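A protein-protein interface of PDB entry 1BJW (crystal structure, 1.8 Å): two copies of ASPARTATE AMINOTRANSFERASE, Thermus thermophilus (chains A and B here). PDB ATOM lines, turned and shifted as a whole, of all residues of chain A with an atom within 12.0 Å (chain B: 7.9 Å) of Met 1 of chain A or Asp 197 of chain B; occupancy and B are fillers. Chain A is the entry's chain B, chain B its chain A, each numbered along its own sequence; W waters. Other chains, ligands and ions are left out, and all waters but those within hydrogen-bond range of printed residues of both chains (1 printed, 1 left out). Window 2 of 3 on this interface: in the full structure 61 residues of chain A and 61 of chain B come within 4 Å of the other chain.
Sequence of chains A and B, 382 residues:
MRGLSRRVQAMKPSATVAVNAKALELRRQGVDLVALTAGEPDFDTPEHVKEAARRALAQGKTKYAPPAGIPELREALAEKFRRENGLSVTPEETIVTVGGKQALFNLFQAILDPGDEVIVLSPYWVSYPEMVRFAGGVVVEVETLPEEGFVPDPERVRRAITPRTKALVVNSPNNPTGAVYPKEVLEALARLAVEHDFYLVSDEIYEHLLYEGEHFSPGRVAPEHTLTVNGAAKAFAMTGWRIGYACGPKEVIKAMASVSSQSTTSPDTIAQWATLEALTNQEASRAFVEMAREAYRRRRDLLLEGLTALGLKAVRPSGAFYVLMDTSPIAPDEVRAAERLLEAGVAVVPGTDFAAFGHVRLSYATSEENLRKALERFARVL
No position is printed for both chains.
Among the printed residues, merely in contact across the chains: Met 1 of chain A with Lys 166 of chain B (3.3 Å), Arg 2 of chain A with Lys 166 of chain B (3.9 Å), Arg 2 of chain A with Phe 198 of chain B (3.8 Å), Arg 2 of chain A with Tyr 199 of chain B (3.7 Å), Gly 3 of chain A with Ile 111 of chain B (3.9 Å), Gly 3 of chain A with Lys 166 of chain B (3.2 Å) and Ser 5 of chain A with Ile 111 of chain B (3.99 Å).
Met 1 of chain A touches just these residues of chain B: Thr 165 (3.4 Å), Lys 166 (3.3 Å) and Asp 197 (2.7 Å).
Of chain A, only Met 1 (2.7 Å) and Arg 2 (3.1 Å) come within 4 Å of Asp 197 of chain B.
Of chain A, only Met 1 (3.4 Å) comes within 4 Å of Thr 165 of chain B.
No residue of chain A comes within 4 Å of Ala 193 of chain B.
Phe 198 of chain B touches one residue of chain A.
Tyr 199 of chain B touches just these residues of chain A: Arg 2 (3.7 Å) and Gly 3 (3.0 Å).
Of the printed residues of chain B, Arg 2 of chain A touches Lys 166, Asp 197, Phe 198, Tyr 199, Glu 224 and His 225.
Of the printed residues of chain B, Gly 3 of chain A touches Ile 111, Lys 166 and Tyr 199.
Of the printed residues of chain A, His 225 of chain B touches Arg 2 (3.3 Å).
Of the printed residues of chain A, Glu 224 of chain B touches Arg 2 (2.9 Å).
Glu 195 of chain B touches none of the printed residues of chain A.
Leu 4 of chain A touches none of the printed residues of chain B.
The nearest residue of chain B that does not touch Met 1 of chain A is Phe 198 of chain B (4.2 Å).
The nearest residue of chain A that does not touch Asp 197 of chain B is Gly 3 of chain A (6.7 Å).
The nearest printed residue of chain B that does not touch Arg 2 of chain A is Ala 193 of chain B (5.8 Å).
Of the 7 printed residues of chain A, 4 touch a printed residue of chain B.
Of the 23 printed residues of chain B, 8 touch a printed residue of chain A.
Printed residues of chain B that touch a printed residue of chain A: Ile 111, Thr 165, Lys 166, Asp 197, Phe 198, Tyr 199, Glu 224 and His 225.
Hydrophobic or aromatic side chains of chain B that line the printed part of chain A: Tyr 199 and His 225.
Along chain B the printed residues that touch a printed residue of chain A span positions 111 to 225.
The backbone NH (N) of Met 1 of chain A is in hydrogen-bond range of the backbone carbonyl oxygen (O) of Thr 165 of chain B (3.4 Å).
NH2 of Arg 2 of chain A lies within hydrogen-bond range of NE2 of His 225 of chain B (3.4 Å).
The backbone carbonyl oxygen (O) of Glu 224 of chain B sits at hydrogen-bond distance from the guanidinium group (NH1) of Arg 2 of chain A, at 2.9 Å.
The side-chain hydroxyl (OH) of Tyr 199 of chain B sits at hydrogen-bond distance from the backbone NH (N) of Gly 3 of chain A (3.0 Å).
OD1 of Asp 197 of chain B is in salt-bridge range of NE of Arg 2 of chain A, at 3.1 Å.
N of Met 1 of chain A sits at hydrogen-bond distance from O of Asp 197 of chain B, at 2.8 Å.
The backbone carbonyl oxygen of Ile 111 of chain B lies within hydrogen-bond range of the side-chain amino group of Lys 166 of chain B, at 2.8 Å.
The backbone NH (N) of Leu 200 of chain B sits at hydrogen-bond distance from the backbone carbonyl oxygen (O) of His 225 of chain B, 2.8 Å away.
The backbone carbonyl oxygen of Ala 193 of chain B lies within hydrogen-bond range of the backbone NH of Phe 198 of chain B (3.1 Å).
The backbone carbonyl oxygen (O) of Lys 166 of chain B sits at hydrogen-bond distance from the backbone NH (N) of Tyr 199 of chain B (2.9 Å).
NZ of Lys 166 of chain B is in salt-bridge range of OD2 of Asp 116 of chain B.
O of Glu 117 of chain B sits at hydrogen-bond distance from N of Lys 166 of chain B, at 2.8 Å.
Water W1 lies within hydrogen-bond range of NH1 of Arg 2 of chain A (2.9 Å) and O of Glu 224 of chain B (3.4 Å).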
ATOM      1  N   MET A   1       7.485   3.941 -11.944  1.00  0.00           N
ATOM      2  CA  MET A   1       7.351   2.505 -12.332  1.00  0.00           C
ATOM      3  C   MET A   1       7.786   2.234 -13.767  1.00  0.00           C
ATOM      4  O   MET A   1       7.802   3.138 -14.602  1.00  0.00           O
ATOM      5  CB  MET A   1       5.902   2.053 -12.175  1.00  0.00           C
ATOM      6  CG  MET A   1       5.760   0.551 -11.945  1.00  0.00           C
ATOM      7  SD  MET A   1       6.656   0.037 -10.437  1.00  0.00           S
ATOM      8  CE  MET A   1       6.498  -1.788 -10.480  1.00  0.00           C
ATOM      9  N   ARG A   2       8.221   1.014 -14.033  1.00  0.00           N
ATOM     10  CA  ARG A   2       8.615   0.651 -15.374  1.00  0.00           C
ATOM     11  C   ARG A   2       7.459  -0.118 -15.974  1.00  0.00           C
ATOM     12  O   ARG A   2       6.435  -0.287 -15.330  1.00  0.00           O
ATOM     13  CB  ARG A   2       9.895  -0.182 -15.374  1.00  0.00           C
ATOM     14  CG  ARG A   2      11.128   0.687 -15.206  1.00  0.00           C
ATOM     15  CD  ARG A   2      12.394  -0.135 -15.221  1.00  0.00           C
ATOM     16  NE  ARG A   2      12.492  -0.965 -14.028  1.00  0.00           N
ATOM     17  CZ  ARG A   2      13.080  -2.153 -14.006  1.00  0.00           C
ATOM     18  NH1 ARG A   2      13.621  -2.633 -15.119  1.00  0.00           N
ATOM     19  NH2 ARG A   2      13.120  -2.867 -12.883  1.00  0.00           N
ATOM     20  N   GLY A   3       7.596  -0.521 -17.234  1.00  0.00           N
ATOM     21  CA  GLY A   3       6.541  -1.292 -17.884  1.00  0.00           C
ATOM     22  C   GLY A   3       6.111  -0.611 -19.163  1.00  0.00           C
ATOM     23  O   GLY A   3       6.225   0.601 -19.318  1.00  0.00           O
ATOM     24  N   LEU A   4       5.557  -1.386 -20.082  1.00  0.00           N
ATOM     25  CA  LEU A   4       5.107  -0.849 -21.351  1.00  0.00           C
ATOM     26  C   LEU A   4       3.791  -0.095 -21.351  1.00  0.00           C
ATOM     27  O   LEU A   4       2.978  -0.217 -20.441  1.00  0.00           O
ATOM     28  CB  LEU A   4       5.048  -1.972 -22.362  1.00  0.00           C
ATOM     29  CG  LEU A   4       6.360  -2.719 -22.448  1.00  0.00           C
ATOM     30  CD1 LEU A   4       6.131  -3.912 -23.359  1.00  0.00           C
ATOM     31  CD2 LEU A   4       7.460  -1.809 -22.968  1.00  0.00           C
ATOM     32  N   SER A   5       3.563   0.681 -22.403  1.00  0.00           N
ATOM     33  CA  SER A   5       2.345   1.443 -22.514  1.00  0.00           C
ATOM     34  C   SER A   5       1.218   0.522 -22.962  1.00  0.00           C
ATOM     35  O   SER A   5       1.449  -0.495 -23.606  1.00  0.00           O
ATOM     36  CB  SER A   5       2.494   2.582 -23.539  1.00  0.00           C
ATOM     37  OG  SER A   5       2.748   2.064 -24.827  1.00  0.00           O
ATOM     38  N   ARG A   6       0.000   0.917 -22.629  1.00  0.00           N
ATOM     39  CA  ARG A   6      -1.194   0.184 -22.996  1.00  0.00           C
ATOM     40  C   ARG A   6      -1.219  -0.024 -24.503  1.00  0.00           C
ATOM     41  O   ARG A   6      -1.354  -1.144 -24.955  1.00  0.00           O
ATOM     42  CB  ARG A   6      -2.426   0.981 -22.590  1.00  0.00           C
ATOM     43  CG  ARG A   6      -2.500   1.195 -21.100  1.00  0.00           C
ATOM     44  CD  ARG A   6      -3.756   1.971 -20.661  1.00  0.00           C
ATOM     45  NE  ARG A   6      -4.186   1.515 -19.330  1.00  0.00           N
ATOM     46  CZ  ARG A   6      -3.743   2.004 -18.168  1.00  0.00           C
ATOM     47  NH1 ARG A   6      -2.855   3.001 -18.149  1.00  0.00           N
ATOM     48  NH2 ARG A   6      -4.129   1.436 -17.019  1.00  0.00           N
ATOM     49  N   GLN A   9       0.946  -2.659 -25.757  1.00  0.00           N
ATOM     50  CA  GLN A   9       0.528  -3.942 -25.221  1.00  0.00           C
ATOM     51  C   GLN A   9      -0.696  -4.522 -25.936  1.00  0.00           C
ATOM     52  O   GLN A   9      -0.869  -5.741 -25.991  1.00  0.00           O
ATOM     53  CB  GLN A   9       0.278  -3.827 -23.723  1.00  0.00           C
ATOM     54  CG  GLN A   9       1.548  -3.619 -22.938  1.00  0.00           C
ATOM     55  CD  GLN A   9       1.376  -3.906 -21.469  1.00  0.00           C
ATOM     56  OE1 GLN A   9       0.944  -3.053 -20.700  1.00  0.00           O
ATOM     57  NE2 GLN A   9       1.732  -5.119 -21.068  1.00  0.00           N
ATOM     58  N   ILE B 111       6.580   3.270 -23.976  1.00  0.00           N
ATOM     59  CA  ILE B 111       6.589   3.282 -22.522  1.00  0.00           C
ATOM     60  C   ILE B 111       5.712   4.313 -21.835  1.00  0.00           C
ATOM     61  O   ILE B 111       5.487   4.219 -20.630  1.00  0.00           O
ATOM     62  CB  ILE B 111       8.033   3.422 -21.974  1.00  0.00           C
ATOM     63  CG1 ILE B 111       8.611   4.797 -22.336  1.00  0.00           C
ATOM     64  CG2 ILE B 111       8.918   2.302 -22.506  1.00  0.00           C
ATOM     65  CD1 ILE B 111       9.889   5.160 -21.556  1.00  0.00           C
ATOM     66  N   ASP B 116       1.911   9.907 -17.485  1.00  0.00           N
ATOM     67  CA  ASP B 116       3.248   9.581 -17.021  1.00  0.00           C
ATOM     68  C   ASP B 116       4.168  10.799 -17.177  1.00  0.00           C
ATOM     69  O   ASP B 116       4.035  11.588 -18.132  1.00  0.00           O
ATOM     70  CB  ASP B 116       3.821   8.393 -17.802  1.00  0.00           C
ATOM     71  CG  ASP B 116       3.080   7.082 -17.526  1.00  0.00           C
ATOM     72  OD1 ASP B 116       2.285   7.000 -16.573  1.00  0.00           O
ATOM     73  OD2 ASP B 116       3.271   6.121 -18.278  1.00  0.00           O
ATOM     74  N   GLU B 117       5.086  10.940 -16.218  1.00  0.00           N
ATOM     75  CA  GLU B 117       6.035  12.037 -16.182  1.00  0.00           C
ATOM     76  C   GLU B 117       7.410  11.629 -16.654  1.00  0.00           C
ATOM     77  O   GLU B 117       7.875  10.523 -16.383  1.00  0.00           O
ATOM     78  CB  GLU B 117       6.117  12.596 -14.773  1.00  0.00           C
ATOM     79  CG  GLU B 117       4.817  13.226 -14.336  1.00  0.00           C
ATOM     80  CD  GLU B 117       4.780  13.566 -12.852  1.00  0.00           C
ATOM     81  OE1 GLU B 117       5.830  13.488 -12.174  1.00  0.00           O
ATOM     82  OE2 GLU B 117       3.679  13.894 -12.360  1.00  0.00           O
ATOM     83  N   ILE B 161      11.323  13.729  -8.604  1.00  0.00           N
ATOM     84  CA  ILE B 161      10.714  12.423  -8.746  1.00  0.00           C
ATOM     85  C   ILE B 161       9.380  12.304  -7.966  1.00  0.00           C
ATOM     86  O   ILE B 161       9.260  12.770  -6.829  1.00  0.00           O
ATOM     87  CB  ILE B 161      11.699  11.354  -8.291  1.00  0.00           C
ATOM     88  CG1 ILE B 161      12.986  11.463  -9.119  1.00  0.00           C
ATOM     89  CG2 ILE B 161      11.054   9.963  -8.355  1.00  0.00           C
ATOM     90  CD1 ILE B 161      14.083  10.496  -8.730  1.00  0.00           C
ATOM     91  N   THR B 162       8.354  11.779  -8.643  1.00  0.00           N
ATOM     92  CA  THR B 162       7.039  11.557  -8.060  1.00  0.00           C
ATOM     93  C   THR B 162       6.666  10.107  -8.364  1.00  0.00           C
ATOM     94  O   THR B 162       7.398   9.392  -9.054  1.00  0.00           O
ATOM     95  CB  THR B 162       5.940  12.460  -8.673  1.00  0.00           C
ATOM     96  OG1 THR B 162       5.535  11.930  -9.936  1.00  0.00           O
ATOM     97  CG2 THR B 162       6.413  13.893  -8.840  1.00  0.00           C
ATOM     98  N   PRO B 163       5.541   9.634  -7.813  1.00  0.00           N
ATOM     99  CA  PRO B 163       5.161   8.247  -8.099  1.00  0.00           C
ATOM    100  C   PRO B 163       4.776   8.058  -9.577  1.00  0.00           C
ATOM    101  O   PRO B 163       4.652   6.913 -10.042  1.00  0.00           O
ATOM    102  CB  PRO B 163       3.960   8.032  -7.174  1.00  0.00           C
ATOM    103  CG  PRO B 163       4.214   8.981  -6.043  1.00  0.00           C
ATOM    104  CD  PRO B 163       4.669  10.208  -6.775  1.00  0.00           C
ATOM    105  N   ARG B 164       4.564   9.184 -10.284  1.00  0.00           N
ATOM    106  CA  ARG B 164       4.195   9.225 -11.721  1.00  0.00           C
ATOM    107  C   ARG B 164       5.423   9.241 -12.668  1.00  0.00           C
ATOM    108  O   ARG B 164       5.265   9.149 -13.886  1.00  0.00           O
ATOM    109  CB  ARG B 164       3.341  10.467 -12.031  1.00  0.00           C
ATOM    110  CG  ARG B 164       2.010  10.595 -11.269  1.00  0.00           C
ATOM    111  CD  ARG B 164       0.800  10.083 -12.066  1.00  0.00           C
ATOM    112  NE  ARG B 164       0.960   8.691 -12.508  1.00  0.00           N
ATOM    113  CZ  ARG B 164       0.542   8.198 -13.682  1.00  0.00           C
ATOM    114  NH1 ARG B 164      -0.083   8.969 -14.574  1.00  0.00           N
ATOM    115  NH2 ARG B 164       0.799   6.928 -13.989  1.00  0.00           N
ATOM    116  N   THR B 165       6.630   9.358 -12.111  1.00  0.00           N
ATOM    117  CA  THR B 165       7.862   9.379 -12.908  1.00  0.00           C
ATOM    118  C   THR B 165       8.134   8.063 -13.625  1.00  0.00           C
ATOM    119  O   THR B 165       8.348   7.036 -12.985  1.00  0.00           O
ATOM    120  CB  THR B 165       9.115   9.724 -12.035  1.00  0.00           C
ATOM    121  OG1 THR B 165       8.931  10.995 -11.405  1.00  0.00           O
ATOM    122  CG2 THR B 165      10.380   9.758 -12.880  1.00  0.00           C
ATOM    123  N   LYS B 166       8.163   8.108 -14.954  1.00  0.00           N
ATOM    124  CA  LYS B 166       8.408   6.927 -15.777  1.00  0.00           C
ATOM    125  C   LYS B 166       9.789   6.936 -16.401  1.00  0.00           C
ATOM    126  O   LYS B 166      10.342   5.871 -16.729  1.00  0.00           O
ATOM    127  CB  LYS B 166       7.361   6.846 -16.881  1.00  0.00           C
ATOM    128  CG  LYS B 166       6.525   5.621 -16.821  1.00  0.00           C
ATOM    129  CD  LYS B 166       7.123   4.468 -17.572  1.00  0.00           C
ATOM    130  CE  LYS B 166       6.167   3.272 -17.507  1.00  0.00           C
ATOM    131  NZ  LYS B 166       4.763   3.567 -17.975  1.00  0.00           N
ATOM    132  N   ALA B 167      10.334   8.135 -16.595  1.00  0.00           N
ATOM    133  CA  ALA B 167      11.637   8.272 -17.201  1.00  0.00           C
ATOM    134  C   ALA B 167      12.363   9.599 -16.908  1.00  0.00           C
ATOM    135  O   ALA B 167      11.749  10.621 -16.593  1.00  0.00           O
ATOM    136  CB  ALA B 167      11.513   8.078 -18.721  1.00  0.00           C
ATOM    137  N   ALA B 190      21.745   7.147 -12.563  1.00  0.00           N
ATOM    138  CA  ALA B 190      21.355   5.768 -12.803  1.00  0.00           C
ATOM    139  C   ALA B 190      20.766   5.184 -11.492  1.00  0.00           C
ATOM    140  O   ALA B 190      19.685   4.563 -11.488  1.00  0.00           O
ATOM    141  CB  ALA B 190      22.571   4.979 -13.231  1.00  0.00           C
ATOM    142  N   ARG B 191      21.467   5.434 -10.377  1.00  0.00           N
ATOM    143  CA  ARG B 191      21.037   4.979  -9.046  1.00  0.00           C
ATOM    144  C   ARG B 191      19.618   5.402  -8.685  1.00  0.00           C
ATOM    145  O   ARG B 191      18.895   4.646  -8.069  1.00  0.00           O
ATOM    146  CB  ARG B 191      21.976   5.487  -7.963  1.00  0.00           C
ATOM    147  CG  ARG B 191      23.285   4.769  -7.907  1.00  0.00           C
ATOM    148  CD  ARG B 191      24.038   5.110  -6.610  1.00  0.00           C
ATOM    149  NE  ARG B 191      25.402   4.590  -6.688  1.00  0.00           N
ATOM    150  CZ  ARG B 191      26.483   5.338  -6.903  1.00  0.00           C
ATOM    151  NH1 ARG B 191      26.379   6.663  -7.045  1.00  0.00           N
ATOM    152  NH2 ARG B 191      27.660   4.744  -7.060  1.00  0.00           N
ATOM    153  N   LEU B 192      19.249   6.632  -9.013  1.00  0.00           N
ATOM    154  CA  LEU B 192      17.911   7.115  -8.741  1.00  0.00           C
ATOM    155  C   LEU B 192      16.888   6.330  -9.530  1.00  0.00           C
ATOM    156  O   LEU B 192      15.758   6.157  -9.076  1.00  0.00           O
ATOM    157  CB  LEU B 192      17.784   8.574  -9.116  1.00  0.00           C
ATOM    158  CG  LEU B 192      18.538   9.539  -8.211  1.00  0.00           C
ATOM    159  CD1 LEU B 192      18.229  10.952  -8.698  1.00  0.00           C
ATOM    160  CD2 LEU B 192      18.106   9.354  -6.757  1.00  0.00           C
ATOM    161  N   ALA B 193      17.277   5.894 -10.723  1.00  0.00           N
ATOM    162  CA  ALA B 193      16.396   5.111 -11.583  1.00  0.00           C
ATOM    163  C   ALA B 193      16.088   3.740 -10.956  1.00  0.00           C
ATOM    164  O   ALA B 193      14.942   3.319 -10.892  1.00  0.00           O
ATOM    165  CB  ALA B 193      17.033   4.924 -12.957  1.00  0.00           C
ATOM    166  N   VAL B 194      17.135   3.045 -10.525  1.00  0.00           N
ATOM    167  CA  VAL B 194      17.013   1.734  -9.912  1.00  0.00           C
ATOM    168  C   VAL B 194      16.265   1.839  -8.590  1.00  0.00           C
ATOM    169  O   VAL B 194      15.368   1.055  -8.309  1.00  0.00           O
ATOM    170  CB  VAL B 194      18.416   1.144  -9.669  1.00  0.00           C
ATOM    171  CG1 VAL B 194      18.339  -0.118  -8.801  1.00  0.00           C
ATOM    172  CG2 VAL B 194      19.088   0.834 -11.000  1.00  0.00           C
ATOM    173  N   GLU B 195      16.614   2.867  -7.825  1.00  0.00           N
ATOM    174  CA  GLU B 195      16.061   3.167  -6.510  1.00  0.00           C
ATOM    175  C   GLU B 195      14.599   3.597  -6.556  1.00  0.00           C
ATOM    176  O   GLU B 195      13.822   3.264  -5.648  1.00  0.00           O
ATOM    177  CB  GLU B 195      16.882   4.290  -5.916  1.00  0.00           C
ATOM    178  CG  GLU B 195      17.064   4.331  -4.450  1.00  0.00           C
ATOM    179  CD  GLU B 195      17.844   5.585  -4.082  1.00  0.00           C
ATOM    180  OE1 GLU B 195      19.094   5.566  -4.213  1.00  0.00           O
ATOM    181  OE2 GLU B 195      17.209   6.612  -3.733  1.00  0.00           O
ATOM    182  N   HIS B 196      14.227   4.380  -7.567  1.00  0.00           N
ATOM    183  CA  HIS B 196      12.845   4.823  -7.683  1.00  0.00           C
ATOM    184  C   HIS B 196      12.036   4.138  -8.770  1.00  0.00           C
ATOM    185  O   HIS B 196      10.909   4.526  -9.055  1.00  0.00           O
ATOM    186  CB  HIS B 196      12.762   6.330  -7.790  1.00  0.00           C
ATOM    187  CG  HIS B 196      13.179   7.017  -6.537  1.00  0.00           C
ATOM    188  ND1 HIS B 196      14.474   6.967  -6.067  1.00  0.00           N
ATOM    189  CD2 HIS B 196      12.476   7.737  -5.633  1.00  0.00           C
ATOM    190  CE1 HIS B 196      14.552   7.632  -4.928  1.00  0.00           C
ATOM    191  NE2 HIS B 196      13.354   8.110  -4.642  1.00  0.00           N
ATOM    192  N   ASP B 197      12.620   3.084  -9.328  1.00  0.00           N
ATOM    193  CA  ASP B 197      11.998   2.253 -10.361  1.00  0.00           C
ATOM    194  C   ASP B 197      11.397   2.962 -11.595  1.00  0.00           C
ATOM    195  O   ASP B 197      10.171   3.062 -11.738  1.00  0.00           O
ATOM    196  CB  ASP B 197      10.960   1.330  -9.720  1.00  0.00           C
ATOM    197  CG  ASP B 197      10.562   0.202 -10.626  1.00  0.00           C
ATOM    198  OD1 ASP B 197      11.461  -0.485 -11.147  1.00  0.00           O
ATOM    199  OD2 ASP B 197       9.353   0.001 -10.827  1.00  0.00           O
ATOM    200  N   PHE B 198      12.263   3.501 -12.441  1.00  0.00           N
ATOM    201  CA  PHE B 198      11.822   4.142 -13.669  1.00  0.00           C
ATOM    202  C   PHE B 198      12.919   3.944 -14.688  1.00  0.00           C
ATOM    203  O   PHE B 198      13.938   3.326 -14.385  1.00  0.00           O
ATOM    204  CB  PHE B 198      11.388   5.632 -13.494  1.00  0.00           C
ATOM    205  CG  PHE B 198      12.436   6.545 -12.879  1.00  0.00           C
ATOM    206  CD1 PHE B 198      13.592   6.901 -13.587  1.00  0.00           C
ATOM    207  CD2 PHE B 198      12.269   7.028 -11.576  1.00  0.00           C
ATOM    208  CE1 PHE B 198      14.588   7.731 -13.000  1.00  0.00           C
ATOM    209  CE2 PHE B 198      13.245   7.850 -10.983  1.00  0.00           C
ATOM    210  CZ  PHE B 198      14.415   8.200 -11.698  1.00  0.00           C
ATOM    211  N   TYR B 199      12.681   4.367 -15.923  1.00  0.00           N
ATOM    212  CA  TYR B 199      13.694   4.204 -16.959  1.00  0.00           C
ATOM    213  C   TYR B 199      14.626   5.407 -17.053  1.00  0.00           C
ATOM    214  O   TYR B 199      14.222   6.547 -16.836  1.00  0.00           O
ATOM    215  CB  TYR B 199      13.044   4.026 -18.329  1.00  0.00           C
ATOM    216  CG  TYR B 199      12.229   2.766 -18.485  1.00  0.00           C
ATOM    217  CD1 TYR B 199      12.852   1.541 -18.709  1.00  0.00           C
ATOM    218  CD2 TYR B 199      10.827   2.818 -18.464  1.00  0.00           C
ATOM    219  CE1 TYR B 199      12.104   0.396 -18.920  1.00  0.00           C
ATOM    220  CE2 TYR B 199      10.067   1.679 -18.668  1.00  0.00           C
ATOM    221  CZ  TYR B 199      10.707   0.472 -18.901  1.00  0.00           C
ATOM    222  OH  TYR B 199       9.947  -0.652 -19.135  1.00  0.00           O
ATOM    223  N   LEU B 200      15.870   5.116 -17.387  1.00  0.00           N
ATOM    224  CA  LEU B 200      16.886   6.131 -17.598  1.00  0.00           C
ATOM    225  C   LEU B 200      17.182   6.084 -19.117  1.00  0.00           C
ATOM    226  O   LEU B 200      17.544   5.035 -19.666  1.00  0.00           O
ATOM    227  CB  LEU B 200      18.115   5.768 -16.764  1.00  0.00           C
ATOM    228  CG  LEU B 200      19.132   6.837 -16.375  1.00  0.00           C
ATOM    229  CD1 LEU B 200      20.461   6.521 -17.003  1.00  0.00           C
ATOM    230  CD2 LEU B 200      18.633   8.209 -16.750  1.00  0.00           C
ATOM    231  N   GLU B 224      19.081  -2.930 -16.722  1.00  0.00           N
ATOM    232  CA  GLU B 224      17.658  -3.277 -16.748  1.00  0.00           C
ATOM    233  C   GLU B 224      16.804  -2.030 -16.758  1.00  0.00           C
ATOM    234  O   GLU B 224      15.650  -2.078 -17.144  1.00  0.00           O
ATOM    235  CB  GLU B 224      17.275  -4.103 -15.504  1.00  0.00           C
ATOM    236  CG  GLU B 224      17.161  -5.620 -15.699  1.00  0.00           C
ATOM    237  CD  GLU B 224      18.501  -6.320 -15.931  1.00  0.00           C
ATOM    238  OE1 GLU B 224      19.166  -6.675 -14.922  1.00  0.00           O
ATOM    239  OE2 GLU B 224      18.874  -6.538 -17.118  1.00  0.00           O
ATOM    240  N   HIS B 225      17.348  -0.925 -16.264  1.00  0.00           N
ATOM    241  CA  HIS B 225      16.594   0.324 -16.238  1.00  0.00           C
ATOM    242  C   HIS B 225      17.001   1.302 -17.344  1.00  0.00           C
ATOM    243  O   HIS B 225      16.338   2.320 -17.502  1.00  0.00           O
ATOM    244  CB  HIS B 225      16.803   1.061 -14.919  1.00  0.00           C
ATOM    245  CG  HIS B 225      16.242   0.355 -13.726  1.00  0.00           C
ATOM    246  ND1 HIS B 225      16.815  -0.781 -13.193  1.00  0.00           N
ATOM    247  CD2 HIS B 225      15.179   0.650 -12.936  1.00  0.00           C
ATOM    248  CE1 HIS B 225      16.134  -1.152 -12.126  1.00  0.00           C
ATOM    249  NE2 HIS B 225      15.137  -0.301 -11.950  1.00  0.00           N
HETATM  250  O   HOH W   1      12.978  -4.176 -17.448  1.00  0.00           O
